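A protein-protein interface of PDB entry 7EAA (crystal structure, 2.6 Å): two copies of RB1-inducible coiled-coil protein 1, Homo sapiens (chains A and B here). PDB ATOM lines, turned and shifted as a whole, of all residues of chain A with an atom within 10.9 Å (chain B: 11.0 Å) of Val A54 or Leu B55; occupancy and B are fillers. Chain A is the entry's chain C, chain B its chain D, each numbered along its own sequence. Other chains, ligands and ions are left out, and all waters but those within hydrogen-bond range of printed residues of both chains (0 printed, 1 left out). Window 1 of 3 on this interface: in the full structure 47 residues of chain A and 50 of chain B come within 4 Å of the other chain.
Phe B51 touches Gln A47 (CE2 to NE2, 3.7 Å).
CD2 of Phe A51 touches CD1 of Phe B51 (3.6 Å).
Val B54 touches Phe A51.
Val A54 touches Leu B55.
CD1 of Leu A55 touches CD2 of Leu B55, 3.6 Å away.
Leu A55 touches Glu B58.
Lys A59 touches Arg B61.
Lys A62 touches Lys B59.
The side-chain amide nitrogen (NE2) of Gln A47 lies within hydrogen-bond range of the side-chain amide oxygen (OE1) of Gln B47, 2.6 Å away.
Of chain A, only Val A54 (3.9 Å) and Leu A55 (3.6 Å) come within 4 Å of Leu B55.
Of chain B, only Phe B51 (3.6 Å) and Val B54 (3.9 Å) come within 4 Å of Phe A51.
Of chain B, only Leu B55 and Glu B58 come within 4 Å of Leu A55.
Glu A58 touches none of the printed residues of chain B.
No residue of chain A comes within 4 Å of Thr B53.
Val B54 touches just one residue of chain A: Phe A51.
No residue of chain A comes within 4 Å of Thr B56.
Glu B58 touches just one residue of chain A: Leu A55.
Printed residues of chain A within 4 Å of Phe B51: Gln A47 and Phe A51.
Of the printed residues of chain A, Gln B47 touches Gln A47.
Printed residues of chain B within 4 Å of Lys A62: Lys B59.
Of the printed residues of chain B, Lys A59 touches Arg B61 (3.1 Å).
Printed residues of chain B within 4 Å of Gln A47: Gln B47 (2.6 Å) and Phe B51 (3.7 Å).
The nearest residue of chain B that does not touch Val A54 is Phe B51 (6.9 Å).
The nearest printed residue of chain B that does not touch Gln A47 is Gln B48 (4.2 Å).
Of the 17 printed residues of chain A, 6 touch a printed residue of chain B.
Hydrophobic or aromatic side chains of chain A within 4 Å of the printed part of chain B: Phe A51, Val A54 and Leu A55.
Of the 17 printed residues of chain B, 7 touch a printed residue of chain A.
Printed residues of chain B that touch a printed residue of chain A: Gln B47, Phe B51, Val B54, Leu B55, Glu B58, Lys B59 and Arg B61.
The side-chain amino group (NZ) of Lys B59 sits at hydrogen-bond distance from the side-chain sulfur (SD) of Met B60 (3.6 Å).
The side-chain amino group (NZ) of Lys A62 is in salt-bridge range of the side-chain carboxylate (OE1) of Glu A58, 3.7 Å away.
OE1 of Glu B63 is in salt-bridge range of NZ of Lys B59 (2.6 Å).
The side-chain carboxylate (OE1) of Glu B58 lies within salt-bridge range of the guanidinium group (NE) of Arg B61, 3.4 Å away.
Gln A47 touches Phe B51, but with the chains exchanged Phe A51 does not touch Gln B47 (6.8 Å).
Phe B51 touches its own counterpart, Phe A51.
Val A54 touches Leu B55, but with the chains exchanged Leu A55 does not touch Val B54 (4.4 Å).
Lys A62 touches Lys B59, but with the chains exchanged Lys A59 does not touch Lys B62 (6.1 Å).
Of the 9 pairs that touch across the chains among the printed residues, 3 have their exchanged pair printed and touching as well.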
ATOM      1  N   GLU A  46      20.997  12.456  24.097  1.00  0.00           N
ATOM      2  CA  GLU A  46      20.639  11.823  22.832  1.00  0.00           C
ATOM      3  C   GLU A  46      21.489  12.365  21.681  1.00  0.00           C
ATOM      4  O   GLU A  46      22.136  11.604  20.951  1.00  0.00           O
ATOM      5  CB  GLU A  46      19.133  12.020  22.581  1.00  0.00           C
ATOM      6  CG  GLU A  46      18.678  12.010  21.108  1.00  0.00           C
ATOM      7  CD  GLU A  46      17.152  12.191  20.919  1.00  0.00           C
ATOM      8  OE1 GLU A  46      16.700  12.443  19.770  1.00  0.00           O
ATOM      9  OE2 GLU A  46      16.408  12.083  21.922  1.00  0.00           O
ATOM     10  N   GLN A  47      21.542  13.683  21.535  1.00  0.00           N
ATOM     11  CA  GLN A  47      22.217  14.262  20.384  1.00  0.00           C
ATOM     12  C   GLN A  47      23.710  13.972  20.388  1.00  0.00           C
ATOM     13  O   GLN A  47      24.322  13.902  19.320  1.00  0.00           O
ATOM     14  CB  GLN A  47      21.972  15.769  20.331  1.00  0.00           C
ATOM     15  CG  GLN A  47      20.517  16.144  20.106  1.00  0.00           C
ATOM     16  CD  GLN A  47      20.035  15.847  18.683  1.00  0.00           C
ATOM     17  OE1 GLN A  47      19.935  14.683  18.265  1.00  0.00           O
ATOM     18  NE2 GLN A  47      19.733  16.904  17.932  1.00  0.00           N
ATOM     19  N   GLN A  48      24.319  13.820  21.563  1.00  0.00           N
ATOM     20  CA  GLN A  48      25.738  13.498  21.593  1.00  0.00           C
ATOM     21  C   GLN A  48      25.975  12.108  21.030  1.00  0.00           C
ATOM     22  O   GLN A  48      26.920  11.895  20.250  1.00  0.00           O
ATOM     23  CB  GLN A  48      26.282  13.617  23.016  1.00  0.00           C
ATOM     24  CG  GLN A  48      26.503  15.052  23.434  1.00  0.00           C
ATOM     25  CD  GLN A  48      27.208  15.213  24.772  1.00  0.00           C
ATOM     26  OE1 GLN A  48      27.585  14.243  25.438  1.00  0.00           O
ATOM     27  NE2 GLN A  48      27.417  16.455  25.155  1.00  0.00           N
ATOM     28  N   THR A  49      25.107  11.154  21.388  1.00  0.00           N
ATOM     29  CA  THR A  49      25.222   9.821  20.817  1.00  0.00           C
ATOM     30  C   THR A  49      24.878   9.826  19.338  1.00  0.00           C
ATOM     31  O   THR A  49      25.593   9.220  18.531  1.00  0.00           O
ATOM     32  CB  THR A  49      24.339   8.829  21.566  1.00  0.00           C
ATOM     33  OG1 THR A  49      24.846   8.682  22.892  1.00  0.00           O
ATOM     34  CG2 THR A  49      24.383   7.448  20.883  1.00  0.00           C
ATOM     35  N   ASN A  50      23.808  10.513  18.948  1.00  0.00           N
ATOM     36  CA  ASN A  50      23.408  10.427  17.551  1.00  0.00           C
ATOM     37  C   ASN A  50      24.465  11.041  16.658  1.00  0.00           C
ATOM     38  O   ASN A  50      24.908  10.418  15.686  1.00  0.00           O
ATOM     39  CB  ASN A  50      22.063  11.095  17.314  1.00  0.00           C
ATOM     40  CG  ASN A  50      20.928  10.446  18.112  1.00  0.00           C
ATOM     41  OD1 ASN A  50      19.965  11.117  18.472  1.00  0.00           O
ATOM     42  ND2 ASN A  50      21.041   9.155  18.384  1.00  0.00           N
ATOM     43  N   PHE A  51      24.921  12.247  16.983  1.00  0.00           N
ATOM     44  CA  PHE A  51      25.881  12.894  16.100  1.00  0.00           C
ATOM     45  C   PHE A  51      27.195  12.106  16.020  1.00  0.00           C
ATOM     46  O   PHE A  51      27.735  11.865  14.931  1.00  0.00           O
ATOM     47  CB  PHE A  51      26.148  14.319  16.548  1.00  0.00           C
ATOM     48  CG  PHE A  51      27.363  14.863  15.933  1.00  0.00           C
ATOM     49  CD1 PHE A  51      28.542  14.925  16.647  1.00  0.00           C
ATOM     50  CD2 PHE A  51      27.357  15.216  14.598  1.00  0.00           C
ATOM     51  CE1 PHE A  51      29.676  15.392  16.071  1.00  0.00           C
ATOM     52  CE2 PHE A  51      28.496  15.688  14.002  1.00  0.00           C
ATOM     53  CZ  PHE A  51      29.668  15.781  14.743  1.00  0.00           C
ATOM     54  N   ASN A  52      27.719  11.702  17.172  1.00  0.00           N
ATOM     55  CA  ASN A  52      29.012  11.042  17.194  1.00  0.00           C
ATOM     56  C   ASN A  52      28.961   9.639  16.617  1.00  0.00           C
ATOM     57  O   ASN A  52      29.958   9.182  16.057  1.00  0.00           O
ATOM     58  CB  ASN A  52      29.557  11.035  18.612  1.00  0.00           C
ATOM     59  CG  ASN A  52      30.089  12.372  18.999  1.00  0.00           C
ATOM     60  OD1 ASN A  52      31.108  12.793  18.478  1.00  0.00           O
ATOM     61  ND2 ASN A  52      29.381  13.080  19.870  1.00  0.00           N
ATOM     62  N   THR A  53      27.830   8.946  16.725  1.00  0.00           N
ATOM     63  CA  THR A  53      27.716   7.654  16.066  1.00  0.00           C
ATOM     64  C   THR A  53      27.729   7.814  14.549  1.00  0.00           C
ATOM     65  O   THR A  53      28.438   7.086  13.840  1.00  0.00           O
ATOM     66  CB  THR A  53      26.440   6.941  16.509  1.00  0.00           C
ATOM     67  OG1 THR A  53      26.560   6.555  17.882  1.00  0.00           O
ATOM     68  CG2 THR A  53      26.234   5.697  15.665  1.00  0.00           C
ATOM     69  N   VAL A  54      26.949   8.762  14.039  1.00  0.00           N
ATOM     70  CA  VAL A  54      26.855   8.934  12.604  1.00  0.00           C
ATOM     71  C   VAL A  54      28.194   9.382  12.042  1.00  0.00           C
ATOM     72  O   VAL A  54      28.631   8.919  10.983  1.00  0.00           O
ATOM     73  CB  VAL A  54      25.719   9.917  12.264  1.00  0.00           C
ATOM     74  CG1 VAL A  54      25.847  10.427  10.830  1.00  0.00           C
ATOM     75  CG2 VAL A  54      24.354   9.262  12.475  1.00  0.00           C
ATOM     76  N   LEU A  55      28.883  10.266  12.750  1.00  0.00           N
ATOM     77  CA  LEU A  55      30.182  10.704  12.274  1.00  0.00           C
ATOM     78  C   LEU A  55      31.190   9.568  12.309  1.00  0.00           C
ATOM     79  O   LEU A  55      31.944   9.371  11.352  1.00  0.00           O
ATOM     80  CB  LEU A  55      30.675  11.878  13.107  1.00  0.00           C
ATOM     81  CG  LEU A  55      31.895  12.505  12.444  1.00  0.00           C
ATOM     82  CD1 LEU A  55      31.403  13.653  11.587  1.00  0.00           C
ATOM     83  CD2 LEU A  55      32.872  12.981  13.472  1.00  0.00           C
ATOM     84  N   THR A  56      31.213   8.798  13.402  1.00  0.00           N
ATOM     85  CA  THR A  56      32.183   7.713  13.508  1.00  0.00           C
ATOM     86  C   THR A  56      31.900   6.600  12.501  1.00  0.00           C
ATOM     87  O   THR A  56      32.831   5.983  11.964  1.00  0.00           O
ATOM     88  CB  THR A  56      32.207   7.181  14.930  1.00  0.00           C
ATOM     89  OG1 THR A  56      32.436   8.277  15.798  1.00  0.00           O
ATOM     90  CG2 THR A  56      33.359   6.232  15.121  1.00  0.00           C
ATOM     91  N   ARG A  57      30.627   6.351  12.201  1.00  0.00           N
ATOM     92  CA  ARG A  57      30.317   5.384  11.159  1.00  0.00           C
ATOM     93  C   ARG A  57      30.792   5.858   9.795  1.00  0.00           C
ATOM     94  O   ARG A  57      31.234   5.043   8.981  1.00  0.00           O
ATOM     95  CB  ARG A  57      28.825   5.085  11.147  1.00  0.00           C
ATOM     96  CG  ARG A  57      28.463   4.121  12.244  1.00  0.00           C
ATOM     97  CD  ARG A  57      26.992   3.874  12.298  1.00  0.00           C
ATOM     98  NE  ARG A  57      26.689   2.936  13.366  1.00  0.00           N
ATOM     99  CZ  ARG A  57      25.469   2.726  13.844  1.00  0.00           C
ATOM    100  NH1 ARG A  57      24.442   3.394  13.338  1.00  0.00           N
ATOM    101  NH2 ARG A  57      25.280   1.849  14.822  1.00  0.00           N
ATOM    102  N   GLU A  58      30.730   7.163   9.530  1.00  0.00           N
ATOM    103  CA  GLU A  58      31.292   7.677   8.284  1.00  0.00           C
ATOM    104  C   GLU A  58      32.812   7.611   8.279  1.00  0.00           C
ATOM    105  O   GLU A  58      33.409   7.296   7.254  1.00  0.00           O
ATOM    106  CB  GLU A  58      30.828   9.105   8.027  1.00  0.00           C
ATOM    107  CG  GLU A  58      29.667   9.196   7.050  1.00  0.00           C
ATOM    108  CD  GLU A  58      29.882   8.381   5.761  1.00  0.00           C
ATOM    109  OE1 GLU A  58      30.644   8.845   4.863  1.00  0.00           O
ATOM    110  OE2 GLU A  58      29.275   7.281   5.653  1.00  0.00           O
ATOM    111  N   LYS A  59      33.467   7.921   9.394  1.00  0.00           N
ATOM    112  CA  LYS A  59      34.910   7.718   9.439  1.00  0.00           C
ATOM    113  C   LYS A  59      35.248   6.286   9.051  1.00  0.00           C
ATOM    114  O   LYS A  59      36.012   6.048   8.112  1.00  0.00           O
ATOM    115  CB  LYS A  59      35.464   8.020  10.832  1.00  0.00           C
ATOM    116  CG  LYS A  59      35.974   9.410  11.057  1.00  0.00           C
ATOM    117  CD  LYS A  59      35.417  10.031  12.375  1.00  0.00           C
ATOM    118  CE  LYS A  59      36.436  10.033  13.524  1.00  0.00           C
ATOM    119  NZ  LYS A  59      36.054  10.967  14.665  1.00  0.00           N
ATOM    120  N   MET A  60      34.630   5.319   9.737  1.00  0.00           N
ATOM    121  CA  MET A  60      35.006   3.922   9.581  1.00  0.00           C
ATOM    122  C   MET A  60      34.755   3.431   8.170  1.00  0.00           C
ATOM    123  O   MET A  60      35.569   2.692   7.609  1.00  0.00           O
ATOM    124  CB  MET A  60      34.254   3.072  10.599  1.00  0.00           C
ATOM    125  CG  MET A  60      34.869   3.209  11.961  1.00  0.00           C
ATOM    126  SD  MET A  60      33.953   2.493  13.335  1.00  0.00           S
ATOM    127  CE  MET A  60      35.238   2.595  14.594  1.00  0.00           C
ATOM    128  N   ARG A  61      33.639   3.843   7.583  1.00  0.00           N
ATOM    129  CA  ARG A  61      33.292   3.439   6.229  1.00  0.00           C
ATOM    130  C   ARG A  61      34.353   3.888   5.239  1.00  0.00           C
ATOM    131  O   ARG A  61      34.783   3.114   4.374  1.00  0.00           O
ATOM    132  CB  ARG A  61      31.936   4.030   5.855  1.00  0.00           C
ATOM    133  CG  ARG A  61      31.240   3.351   4.719  1.00  0.00           C
ATOM    134  CD  ARG A  61      29.978   4.101   4.310  1.00  0.00           C
ATOM    135  NE  ARG A  61      29.985   4.223   2.866  1.00  0.00           N
ATOM    136  CZ  ARG A  61      30.005   5.374   2.219  1.00  0.00           C
ATOM    137  NH1 ARG A  61      29.963   6.502   2.909  1.00  0.00           N
ATOM    138  NH2 ARG A  61      30.049   5.391   0.888  1.00  0.00           N
ATOM    139  N   LYS A  62      34.794   5.145   5.354  1.00  0.00           N
ATOM    140  CA  LYS A  62      35.756   5.664   4.392  1.00  0.00           C
ATOM    141  C   LYS A  62      37.133   5.081   4.642  1.00  0.00           C
ATOM    142  O   LYS A  62      37.879   4.815   3.689  1.00  0.00           O
ATOM    143  CB  LYS A  62      35.786   7.196   4.429  1.00  0.00           C
ATOM    144  CG  LYS A  62      34.456   7.821   4.047  1.00  0.00           C
ATOM    145  CD  LYS A  62      34.664   9.065   3.230  1.00  0.00           C
ATOM    146  CE  LYS A  62      33.340   9.628   2.722  1.00  0.00           C
ATOM    147  NZ  LYS A  62      32.705   8.729   1.737  1.00  0.00           N
ATOM    148  N   GLN B  47      20.080  21.686  15.687  1.00  0.00           N
ATOM    149  CA  GLN B  47      21.252  20.815  15.795  1.00  0.00           C
ATOM    150  C   GLN B  47      21.369  19.934  14.565  1.00  0.00           C
ATOM    151  O   GLN B  47      22.414  19.903  13.899  1.00  0.00           O
ATOM    152  CB  GLN B  47      21.182  19.943  17.044  1.00  0.00           C
ATOM    153  CG  GLN B  47      21.528  20.630  18.346  1.00  0.00           C
ATOM    154  CD  GLN B  47      20.730  20.036  19.510  1.00  0.00           C
ATOM    155  OE1 GLN B  47      20.084  18.991  19.368  1.00  0.00           O
ATOM    156  NE2 GLN B  47      20.765  20.709  20.666  1.00  0.00           N
ATOM    157  N   GLN B  48      20.276  19.242  14.227  1.00  0.00           N
ATOM    158  CA  GLN B  48      20.304  18.299  13.124  1.00  0.00           C
ATOM    159  C   GLN B  48      20.717  18.969  11.818  1.00  0.00           C
ATOM    160  O   GLN B  48      21.430  18.357  11.007  1.00  0.00           O
ATOM    161  CB  GLN B  48      18.949  17.605  13.013  1.00  0.00           C
ATOM    162  CG  GLN B  48      18.877  16.310  13.839  1.00  0.00           C
ATOM    163  CD  GLN B  48      17.487  15.690  13.838  1.00  0.00           C
ATOM    164  OE1 GLN B  48      16.666  15.963  12.956  1.00  0.00           O
ATOM    165  NE2 GLN B  48      17.211  14.857  14.839  1.00  0.00           N
ATOM    166  N   THR B  49      20.316  20.224  11.613  1.00  0.00           N
ATOM    167  CA  THR B  49      20.854  21.009  10.503  1.00  0.00           C
ATOM    168  C   THR B  49      22.371  21.157  10.614  1.00  0.00           C
ATOM    169  O   THR B  49      23.102  20.956   9.637  1.00  0.00           O
ATOM    170  CB  THR B  49      20.197  22.398  10.465  1.00  0.00           C
ATOM    171  OG1 THR B  49      18.768  22.277  10.490  1.00  0.00           O
ATOM    172  CG2 THR B  49      20.623  23.171   9.222  1.00  0.00           C
ATOM    173  N   ASN B  50      22.863  21.529  11.798  1.00  0.00           N
ATOM    174  CA  ASN B  50      24.289  21.800  11.938  1.00  0.00           C
ATOM    175  C   ASN B  50      25.109  20.525  11.746  1.00  0.00           C
ATOM    176  O   ASN B  50      26.140  20.549  11.064  1.00  0.00           O
ATOM    177  CB  ASN B  50      24.573  22.434  13.306  1.00  0.00           C
ATOM    178  CG  ASN B  50      24.005  23.847  13.435  1.00  0.00           C
ATOM    179  OD1 ASN B  50      23.910  24.591  12.453  1.00  0.00           O
ATOM    180  ND2 ASN B  50      23.632  24.224  14.662  1.00  0.00           N
ATOM    181  N   PHE B  51      24.653  19.404  12.341  1.00  0.00           N
ATOM    182  CA  PHE B  51      25.270  18.100  12.100  1.00  0.00           C
ATOM    183  C   PHE B  51      25.486  17.894  10.623  1.00  0.00           C
ATOM    184  O   PHE B  51      26.545  17.415  10.193  1.00  0.00           O
ATOM    185  CB  PHE B  51      24.396  16.955  12.625  1.00  0.00           C
ATOM    186  CG  PHE B  51      24.133  16.995  14.104  1.00  0.00           C
ATOM    187  CD1 PHE B  51      24.889  17.800  14.941  1.00  0.00           C
ATOM    188  CD2 PHE B  51      23.121  16.220  14.653  1.00  0.00           C
ATOM    189  CE1 PHE B  51      24.634  17.855  16.281  1.00  0.00           C
ATOM    190  CE2 PHE B  51      22.863  16.260  16.015  1.00  0.00           C
ATOM    191  CZ  PHE B  51      23.618  17.085  16.828  1.00  0.00           C
ATOM    192  N   ASN B  52      24.502  18.300   9.825  1.00  0.00           N
ATOM    193  CA  ASN B  52      24.574  18.062   8.393  1.00  0.00           C
ATOM    194  C   ASN B  52      25.736  18.820   7.767  1.00  0.00           C
ATOM    195  O   ASN B  52      26.492  18.252   6.979  1.00  0.00           O
ATOM    196  CB  ASN B  52      23.242  18.427   7.754  1.00  0.00           C
ATOM    197  CG  ASN B  52      23.104  17.883   6.368  1.00  0.00           C
ATOM    198  OD1 ASN B  52      23.712  16.862   6.024  1.00  0.00           O
ATOM    199  ND2 ASN B  52      22.308  18.558   5.546  1.00  0.00           N
ATOM    200  N   THR B  53      25.913  20.091   8.127  1.00  0.00           N
ATOM    201  CA  THR B  53      27.054  20.858   7.630  1.00  0.00           C
ATOM    202  C   THR B  53      28.365  20.175   7.986  1.00  0.00           C
ATOM    203  O   THR B  53      29.260  20.033   7.139  1.00  0.00           O
ATOM    204  CB  THR B  53      27.050  22.260   8.233  1.00  0.00           C
ATOM    205  OG1 THR B  53      25.705  22.752   8.350  1.00  0.00           O
ATOM    206  CG2 THR B  53      27.846  23.177   7.348  1.00  0.00           C
ATOM    207  N   VAL B  54      28.482  19.739   9.241  1.00  0.00           N
ATOM    208  CA  VAL B  54      29.686  19.070   9.715  1.00  0.00           C
ATOM    209  C   VAL B  54      29.954  17.793   8.934  1.00  0.00           C
ATOM    210  O   VAL B  54      31.086  17.527   8.528  1.00  0.00           O
ATOM    211  CB  VAL B  54      29.568  18.796  11.220  1.00  0.00           C
ATOM    212  CG1 VAL B  54      30.748  17.965  11.701  1.00  0.00           C
ATOM    213  CG2 VAL B  54      29.499  20.102  11.937  1.00  0.00           C
ATOM    214  N   LEU B  55      28.929  16.961   8.741  1.00  0.00           N
ATOM    215  CA  LEU B  55      29.157  15.712   8.018  1.00  0.00           C
ATOM    216  C   LEU B  55      29.577  15.980   6.595  1.00  0.00           C
ATOM    217  O   LEU B  55      30.441  15.276   6.053  1.00  0.00           O
ATOM    218  CB  LEU B  55      27.916  14.832   8.007  1.00  0.00           C
ATOM    219  CG  LEU B  55      27.244  14.497   9.327  1.00  0.00           C
ATOM    220  CD1 LEU B  55      25.828  13.969   9.056  1.00  0.00           C
ATOM    221  CD2 LEU B  55      28.088  13.536  10.162  1.00  0.00           C
ATOM    222  N   THR B  56      28.967  16.984   5.959  1.00  0.00           N
ATOM    223  CA  THR B  56      29.349  17.294   4.584  1.00  0.00           C
ATOM    224  C   THR B  56      30.765  17.813   4.513  1.00  0.00           C
ATOM    225  O   THR B  56      31.516  17.463   3.598  1.00  0.00           O
ATOM    226  CB  THR B  56      28.427  18.320   3.965  1.00  0.00           C
ATOM    227  OG1 THR B  56      27.071  18.043   4.337  1.00  0.00           O
ATOM    228  CG2 THR B  56      28.594  18.246   2.487  1.00  0.00           C
ATOM    229  N   ARG B  57      31.138  18.667   5.462  1.00  0.00           N
ATOM    230  CA  ARG B  57      32.526  19.090   5.562  1.00  0.00           C
ATOM    231  C   ARG B  57      33.457  17.876   5.660  1.00  0.00           C
ATOM    232  O   ARG B  57      34.460  17.792   4.946  1.00  0.00           O
ATOM    233  CB  ARG B  57      32.657  20.043   6.748  1.00  0.00           C
ATOM    234  CG  ARG B  57      34.061  20.367   7.142  1.00  0.00           C
ATOM    235  CD  ARG B  57      34.656  21.472   6.312  1.00  0.00           C
ATOM    236  NE  ARG B  57      35.454  22.362   7.156  1.00  0.00           N
ATOM    237  CZ  ARG B  57      36.748  22.627   6.971  1.00  0.00           C
ATOM    238  NH1 ARG B  57      37.412  22.079   5.959  1.00  0.00           N
ATOM    239  NH2 ARG B  57      37.375  23.453   7.801  1.00  0.00           N
ATOM    240  N   GLU B  58      33.098  16.891   6.497  1.00  0.00           N
ATOM    241  CA  GLU B  58      33.951  15.715   6.701  1.00  0.00           C
ATOM    242  C   GLU B  58      33.948  14.770   5.510  1.00  0.00           C
ATOM    243  O   GLU B  58      34.924  14.034   5.315  1.00  0.00           O
ATOM    244  CB  GLU B  58      33.513  14.918   7.933  1.00  0.00           C
ATOM    245  CG  GLU B  58      33.609  15.679   9.238  1.00  0.00           C
ATOM    246  CD  GLU B  58      34.942  16.391   9.402  1.00  0.00           C
ATOM    247  OE1 GLU B  58      35.983  15.690   9.470  1.00  0.00           O
ATOM    248  OE2 GLU B  58      34.933  17.655   9.446  1.00  0.00           O
ATOM    249  N   LYS B  59      32.848  14.723   4.748  1.00  0.00           N
ATOM    250  CA  LYS B  59      32.812  13.886   3.554  1.00  0.00           C
ATOM    251  C   LYS B  59      33.960  14.222   2.612  1.00  0.00           C
ATOM    252  O   LYS B  59      34.610  13.327   2.064  1.00  0.00           O
ATOM    253  CB  LYS B  59      31.464  14.053   2.852  1.00  0.00           C
ATOM    254  CG  LYS B  59      31.423  13.563   1.405  1.00  0.00           C
ATOM    255  CD  LYS B  59      30.070  13.890   0.737  1.00  0.00           C
ATOM    256  CE  LYS B  59      29.983  13.259  -0.655  1.00  0.00           C
ATOM    257  NZ  LYS B  59      31.330  13.223  -1.333  1.00  0.00           N
ATOM    258  N   MET B  60      34.265  15.508   2.465  1.00  0.00           N
ATOM    259  CA  MET B  60      35.258  15.941   1.492  1.00  0.00           C
ATOM    260  C   MET B  60      36.700  15.785   1.960  1.00  0.00           C
ATOM    261  O   MET B  60      37.598  15.770   1.114  1.00  0.00           O
ATOM    262  CB  MET B  60      34.999  17.399   1.109  1.00  0.00           C
ATOM    263  CG  MET B  60      33.714  17.583   0.311  1.00  0.00           C
ATOM    264  SD  MET B  60      33.374  16.156  -0.769  1.00  0.00           S
ATOM    265  CE  MET B  60      33.911  16.761  -2.374  1.00  0.00           C
ATOM    266  N   ARG B  61      36.959  15.664   3.262  1.00  0.00           N
ATOM    267  CA  ARG B  61      38.348  15.672   3.726  1.00  0.00           C
ATOM    268  C   ARG B  61      39.158  14.507   3.169  1.00  0.00           C
ATOM    269  O   ARG B  61      40.391  14.572   3.158  1.00  0.00           O
ATOM    270  CB  ARG B  61      38.423  15.668   5.260  1.00  0.00           C
ATOM    271  CG  ARG B  61      38.227  14.293   5.903  1.00  0.00           C
ATOM    272  CD  ARG B  61      37.736  14.400   7.359  1.00  0.00           C
ATOM    273  NE  ARG B  61      37.727  13.106   8.052  1.00  0.00           N
ATOM    274  CZ  ARG B  61      36.768  12.186   7.932  1.00  0.00           C
ATOM    275  NH1 ARG B  61      35.712  12.398   7.154  1.00  0.00           N
ATOM    276  NH2 ARG B  61      36.869  11.041   8.588  1.00  0.00           N
ATOM    277  N   LYS B  62      38.498  13.449   2.700  1.00  0.00           N
ATOM    278  CA  LYS B  62      39.180  12.294   2.129  1.00  0.00           C
ATOM    279  C   LYS B  62      38.693  11.981   0.721  1.00  0.00           C
ATOM    280  O   LYS B  62      39.063  10.940   0.164  1.00  0.00           O
ATOM    281  CB  LYS B  62      38.993  11.070   3.030  1.00  0.00           C
ATOM    282  CG  LYS B  62      40.027  10.943   4.125  1.00  0.00           C
ATOM    283  CD  LYS B  62      39.788   9.701   4.951  1.00  0.00           C
ATOM    284  CE  LYS B  62      40.910   9.492   5.956  1.00  0.00           C
ATOM    285  NZ  LYS B  62      41.104  10.668   6.860  1.00  0.00           N
ATOM    286  N   GLU B  63      37.860  12.849   0.141  1.00  0.00           N
ATOM    287  CA  GLU B  63      37.325  12.611  -1.196  1.00  0.00           C
ATOM    288  C   GLU B  63      38.429  12.560  -2.254  1.00  0.00           C
ATOM    289  O   GLU B  63      38.351  11.771  -3.203  1.00  0.00           O
ATOM    290  CB  GLU B  63      36.301  13.696  -1.535  1.00  0.00           C
ATOM    291  CG  GLU B  63      35.707  13.587  -2.923  1.00  0.00           C
ATOM    292  CD  GLU B  63      34.324  12.959  -2.913  1.00  0.00           C
ATOM    293  OE1 GLU B  63      33.800  12.710  -1.801  1.00  0.00           O
ATOM    294  OE2 GLU B  63      33.766  12.720  -4.015  1.00  0.00           O
